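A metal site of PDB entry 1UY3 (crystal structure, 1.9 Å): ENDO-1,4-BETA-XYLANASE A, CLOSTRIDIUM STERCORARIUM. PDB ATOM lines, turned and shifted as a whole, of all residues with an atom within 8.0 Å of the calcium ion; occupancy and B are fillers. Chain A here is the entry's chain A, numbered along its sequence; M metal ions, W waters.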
ATOM      1  N   ILE A  23     -23.424  29.101 -16.695  1.00  0.00           N
ATOM      2  CA  ILE A  23     -22.921  27.754 -16.514  1.00  0.00           C
ATOM      3  C   ILE A  23     -23.050  27.375 -15.036  1.00  0.00           C
ATOM      4  O   ILE A  23     -22.671  28.176 -14.094  1.00  0.00           O
ATOM      5  CB  ILE A  23     -21.447  27.652 -16.947  1.00  0.00           C
ATOM      6  CG1 ILE A  23     -21.294  27.718 -18.469  1.00  0.00           C
ATOM      7  CG2 ILE A  23     -20.764  26.374 -16.371  1.00  0.00           C
ATOM      8  CD1 ILE A  23     -21.877  26.607 -19.270  1.00  0.00           C
ATOM      9  N   ILE A  24     -23.583  26.184 -14.812  1.00  0.00           N
ATOM     10  CA  ILE A  24     -23.672  25.585 -13.466  1.00  0.00           C
ATOM     11  C   ILE A  24     -22.694  24.435 -13.469  1.00  0.00           C
ATOM     12  O   ILE A  24     -22.727  23.582 -14.328  1.00  0.00           O
ATOM     13  CB  ILE A  24     -25.107  25.124 -13.161  1.00  0.00           C
ATOM     14  CG1 ILE A  24     -26.046  26.341 -13.163  1.00  0.00           C
ATOM     15  CG2 ILE A  24     -25.225  24.396 -11.788  1.00  0.00           C
ATOM     16  CD1 ILE A  24     -27.555  25.945 -13.323  1.00  0.00           C
ATOM     17  N   GLU A  25     -21.776  24.424 -12.515  1.00  0.00           N
ATOM     18  CA  GLU A  25     -20.770  23.349 -12.405  1.00  0.00           C
ATOM     19  C   GLU A  25     -21.369  22.148 -11.675  1.00  0.00           C
ATOM     20  O   GLU A  25     -21.910  22.285 -10.576  1.00  0.00           O
ATOM     21  CB  GLU A  25     -19.533  23.873 -11.670  1.00  0.00           C
ATOM     22  CG  GLU A  25     -18.846  25.011 -12.405  1.00  0.00           C
ATOM     23  CD  GLU A  25     -18.220  24.605 -13.712  1.00  0.00           C
ATOM     24  OE1 GLU A  25     -18.175  23.380 -14.032  1.00  0.00           O
ATOM     25  OE2 GLU A  25     -17.742  25.494 -14.416  1.00  0.00           O
ATOM     26  N   ALA A  26     -21.271  20.983 -12.290  1.00  0.00           N
ATOM     27  CA  ALA A  26     -21.918  19.805 -11.753  1.00  0.00           C
ATOM     28  C   ALA A  26     -21.333  19.427 -10.377  1.00  0.00           C
ATOM     29  O   ALA A  26     -22.054  18.918  -9.492  1.00  0.00           O
ATOM     30  CB  ALA A  26     -21.834  18.686 -12.689  1.00  0.00           C
ATOM     31  N   GLU A  27     -20.044  19.645 -10.235  1.00  0.00           N
ATOM     32  CA  GLU A  27     -19.314  19.341  -9.017  1.00  0.00           C
ATOM     33  C   GLU A  27     -19.692  20.233  -7.865  1.00  0.00           C
ATOM     34  O   GLU A  27     -19.375  19.934  -6.736  1.00  0.00           O
ATOM     35  CB  GLU A  27     -17.762  19.387  -9.242  1.00  0.00           C
ATOM     36  CG  GLU A  27     -17.197  20.781  -9.620  1.00  0.00           C
ATOM     37  CD  GLU A  27     -17.219  21.050 -11.100  1.00  0.00           C
ATOM     38  OE1 GLU A  27     -18.059  20.408 -11.830  1.00  0.00           O
ATOM     39  OE2 GLU A  27     -16.394  21.911 -11.570  1.00  0.00           O
ATOM     40  N   GLU A  28     -20.412  21.318  -8.125  1.00  0.00           N
ATOM     41  CA  GLU A  28     -20.884  22.196  -7.089  1.00  0.00           C
ATOM     42  C   GLU A  28     -22.362  21.901  -6.754  1.00  0.00           C
ATOM     43  O   GLU A  28     -23.200  22.761  -6.746  1.00  0.00           O
ATOM     44  CB  GLU A  28     -20.675  23.659  -7.501  1.00  0.00           C
ATOM     45  CG  GLU A  28     -19.177  23.985  -7.684  1.00  0.00           C
ATOM     46  CD  GLU A  28     -18.918  25.403  -8.102  1.00  0.00           C
ATOM     47  OE1 GLU A  28     -17.727  25.710  -8.246  1.00  0.00           O
ATOM     48  OE2 GLU A  28     -19.856  26.203  -8.322  1.00  0.00           O
ATOM     49  N   VAL A  39     -16.025  13.798  -6.956  1.00  0.00           N
ATOM     50  CA  VAL A  39     -15.590  14.937  -7.768  1.00  0.00           C
ATOM     51  C   VAL A  39     -14.364  14.451  -8.535  1.00  0.00           C
ATOM     52  O   VAL A  39     -13.425  13.857  -7.940  1.00  0.00           O
ATOM     53  CB  VAL A  39     -15.339  16.159  -6.948  1.00  0.00           C
ATOM     54  CG1 VAL A  39     -14.678  17.298  -7.765  1.00  0.00           C
ATOM     55  CG2 VAL A  39     -16.657  16.642  -6.357  1.00  0.00           C
ATOM     56  N   ILE A  40     -14.444  14.528  -9.862  1.00  0.00           N
ATOM     57  CA  ILE A  40     -13.385  14.053 -10.751  1.00  0.00           C
ATOM     58  C   ILE A  40     -12.727  15.266 -11.467  1.00  0.00           C
ATOM     59  O   ILE A  40     -13.289  16.347 -11.526  1.00  0.00           O
ATOM     60  CB  ILE A  40     -13.944  13.034 -11.759  1.00  0.00           C
ATOM     61  CG1 ILE A  40     -15.105  13.607 -12.580  1.00  0.00           C
ATOM     62  CG2 ILE A  40     -14.380  11.766 -11.009  1.00  0.00           C
ATOM     63  CD1 ILE A  40     -15.340  12.942 -13.821  1.00  0.00           C
ATOM     64  N   THR A  42     -11.055  16.717 -15.197  1.00  0.00           N
ATOM     65  CA  THR A  42     -11.275  16.560 -16.628  1.00  0.00           C
ATOM     66  C   THR A  42      -9.975  16.838 -17.357  1.00  0.00           C
ATOM     67  O   THR A  42      -9.043  17.342 -16.753  1.00  0.00           O
ATOM     68  CB  THR A  42     -12.362  17.536 -17.156  1.00  0.00           C
ATOM     69  OG1 THR A  42     -11.910  18.893 -16.991  1.00  0.00           O
ATOM     70  CG2 THR A  42     -13.681  17.411 -16.356  1.00  0.00           C
ATOM     71  N   GLY A  46     -10.345  20.901 -15.496  1.00  0.00           N
ATOM     72  CA  GLY A  46     -11.594  21.303 -14.852  1.00  0.00           C
ATOM     73  C   GLY A  46     -12.017  20.191 -13.918  1.00  0.00           C
ATOM     74  O   GLY A  46     -11.220  19.317 -13.599  1.00  0.00           O
ATOM     75  N   ARG A  47     -13.246  20.257 -13.429  1.00  0.00           N
ATOM     76  CA  ARG A  47     -13.789  19.195 -12.573  1.00  0.00           C
ATOM     77  C   ARG A  47     -15.204  18.832 -13.017  1.00  0.00           C
ATOM     78  O   ARG A  47     -15.816  19.536 -13.808  1.00  0.00           O
ATOM     79  CB  ARG A  47     -13.762  19.602 -11.110  1.00  0.00           C
ATOM     80  CG  ARG A  47     -12.358  20.068 -10.605  1.00  0.00           C
ATOM     81  CD  ARG A  47     -12.216  20.219  -9.099  1.00  0.00           C
ATOM     82  NE  ARG A  47     -11.560  19.017  -8.544  1.00  0.00           N
ATOM     83  CZ  ARG A  47     -11.557  18.633  -7.228  1.00  0.00           C
ATOM     84  NH1 ARG A  47     -12.154  19.378  -6.283  1.00  0.00           N
ATOM     85  NH2 ARG A  47     -10.922  17.497  -6.863  1.00  0.00           N
ATOM     86  N   GLY A  48     -15.663  17.702 -12.516  1.00  0.00           N
ATOM     87  CA  GLY A  48     -17.004  17.240 -12.736  1.00  0.00           C
ATOM     88  C   GLY A  48     -17.387  16.251 -11.667  1.00  0.00           C
ATOM     89  O   GLY A  48     -16.732  16.152 -10.622  1.00  0.00           O
ATOM     90  N   ILE A  49     -18.475  15.552 -11.934  1.00  0.00           N
ATOM     91  CA  ILE A  49     -18.895  14.482 -11.109  1.00  0.00           C
ATOM     92  C   ILE A  49     -18.851  13.211 -11.900  1.00  0.00           C
ATOM     93  O   ILE A  49     -19.143  13.199 -13.093  1.00  0.00           O
ATOM     94  CB  ILE A  49     -20.284  14.714 -10.458  1.00  0.00           C
ATOM     95  CG1 ILE A  49     -21.355  14.987 -11.549  1.00  0.00           C
ATOM     96  CG2 ILE A  49     -20.199  15.833  -9.490  1.00  0.00           C
ATOM     97  CD1 ILE A  49     -22.796  15.027 -11.085  1.00  0.00           C
ATOM     98  N   THR A  75     -22.615  19.089 -20.455  1.00  0.00           N
ATOM     99  CA  THR A  75     -21.353  18.607 -21.019  1.00  0.00           C
ATOM    100  C   THR A  75     -20.964  17.339 -20.283  1.00  0.00           C
ATOM    101  O   THR A  75     -20.690  17.366 -19.070  1.00  0.00           O
ATOM    102  CB  THR A  75     -20.285  19.735 -20.926  1.00  0.00           C
ATOM    103  OG1 THR A  75     -20.713  20.893 -21.727  1.00  0.00           O
ATOM    104  CG2 THR A  75     -18.974  19.293 -21.486  1.00  0.00           C
ATOM    105  N   TYR A 110     -15.661  14.516 -23.599  1.00  0.00           N
ATOM    106  CA  TYR A 110     -16.887  15.298 -23.308  1.00  0.00           C
ATOM    107  C   TYR A 110     -17.595  15.834 -24.550  1.00  0.00           C
ATOM    108  O   TYR A 110     -16.976  16.122 -25.545  1.00  0.00           O
ATOM    109  CB  TYR A 110     -16.561  16.400 -22.314  1.00  0.00           C
ATOM    110  CG  TYR A 110     -16.287  15.852 -20.942  1.00  0.00           C
ATOM    111  CD1 TYR A 110     -15.035  15.309 -20.636  1.00  0.00           C
ATOM    112  CD2 TYR A 110     -17.301  15.767 -19.980  1.00  0.00           C
ATOM    113  CE1 TYR A 110     -14.761  14.760 -19.383  1.00  0.00           C
ATOM    114  CE2 TYR A 110     -17.042  15.191 -18.689  1.00  0.00           C
ATOM    115  CZ  TYR A 110     -15.771  14.688 -18.411  1.00  0.00           C
ATOM    116  OH  TYR A 110     -15.442  14.138 -17.185  1.00  0.00           O
ATOM    117  N   VAL A 136     -20.186  14.229 -15.633  1.00  0.00           N
ATOM    118  CA  VAL A 136     -20.826  15.513 -15.964  1.00  0.00           C
ATOM    119  C   VAL A 136     -19.924  16.614 -15.513  1.00  0.00           C
ATOM    120  O   VAL A 136     -19.564  16.673 -14.314  1.00  0.00           O
ATOM    121  CB  VAL A 136     -22.189  15.670 -15.283  1.00  0.00           C
ATOM    122  CG1 VAL A 136     -22.924  16.885 -15.843  1.00  0.00           C
ATOM    123  CG2 VAL A 136     -23.079  14.384 -15.386  1.00  0.00           C
ATOM    124  N   ASP A 137     -19.560  17.512 -16.444  1.00  0.00           N
ATOM    125  CA  ASP A 137     -18.713  18.622 -16.157  1.00  0.00           C
ATOM    126  C   ASP A 137     -19.564  19.824 -15.692  1.00  0.00           C
ATOM    127  O   ASP A 137     -19.346  20.395 -14.595  1.00  0.00           O
ATOM    128  CB  ASP A 137     -17.858  18.933 -17.416  1.00  0.00           C
ATOM    129  CG  ASP A 137     -16.898  20.042 -17.211  1.00  0.00           C
ATOM    130  OD1 ASP A 137     -17.084  20.898 -16.306  1.00  0.00           O
ATOM    131  OD2 ASP A 137     -15.912  20.160 -17.954  1.00  0.00           O
ATOM    132  N   ASN A 138     -20.550  20.162 -16.516  1.00  0.00           N
ATOM    133  CA  ASN A 138     -21.377  21.349 -16.291  1.00  0.00           C
ATOM    134  C   ASN A 138     -22.698  21.222 -17.034  1.00  0.00           C
ATOM    135  O   ASN A 138     -22.907  20.272 -17.777  1.00  0.00           O
ATOM    136  CB  ASN A 138     -20.609  22.628 -16.667  1.00  0.00           C
ATOM    137  CG  ASN A 138     -20.381  22.776 -18.162  1.00  0.00           C
ATOM    138  OD1 ASN A 138     -19.366  23.356 -18.604  1.00  0.00           O
ATOM    139  ND2 ASN A 138     -21.332  22.327 -18.937  1.00  0.00           N
ATOM    140  N   PHE A 139     -23.593  22.159 -16.788  1.00  0.00           N
ATOM    141  CA  PHE A 139     -24.847  22.281 -17.523  1.00  0.00           C
ATOM    142  C   PHE A 139     -25.376  23.706 -17.474  1.00  0.00           C
ATOM    143  O   PHE A 139     -24.884  24.559 -16.734  1.00  0.00           O
ATOM    144  CB  PHE A 139     -25.902  21.259 -17.042  1.00  0.00           C
ATOM    145  CG  PHE A 139     -26.179  21.295 -15.536  1.00  0.00           C
ATOM    146  CD1 PHE A 139     -25.496  20.469 -14.642  1.00  0.00           C
ATOM    147  CD2 PHE A 139     -27.150  22.131 -15.057  1.00  0.00           C
ATOM    148  CE1 PHE A 139     -25.788  20.466 -13.299  1.00  0.00           C
ATOM    149  CE2 PHE A 139     -27.424  22.167 -13.711  1.00  0.00           C
ATOM    150  CZ  PHE A 139     -26.741  21.341 -12.827  1.00  0.00           C
HETATM  151 CA    CA M   1     -17.183  21.360 -14.009  1.00  0.00          CA
HETATM  152  O   HOH W   1     -15.004  22.474 -14.373  1.00  0.00           O
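Within 4 Å of the calcium ion: Glu 25, Glu 27, Arg 47 and Asp 137. The nearest printed residue that does not touch the calcium ion is Gly 48 (4.2 Å).
O of Asp 137 lies close to N of Ala 26 (3.1 Å). The backbone carbonyl oxygen (O) of Thr 75 is in hydrogen-bond range of the backbone NH (N) of Asp 137 (2.9 Å).
The calcium ion is bound by OE1 of Glu 25 (2.3 Å). The backbone carbonyl oxygen (O) of Arg 47 binds the calcium ion (2.3 Å). The calcium ion is bound by the side-chain carboxylate (OD1) of Asp 137. The calcium ion is bound by O of Asp 137. Water W1 is bound to the calcium ion (2.5 Å). The calcium ion is bound by the side-chain carboxylate (OE1) of Glu 27, at 2.5 Å. The calcium ion is bound by the side-chain carboxylate (OE2) of Glu 27, at 2.6 Å.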
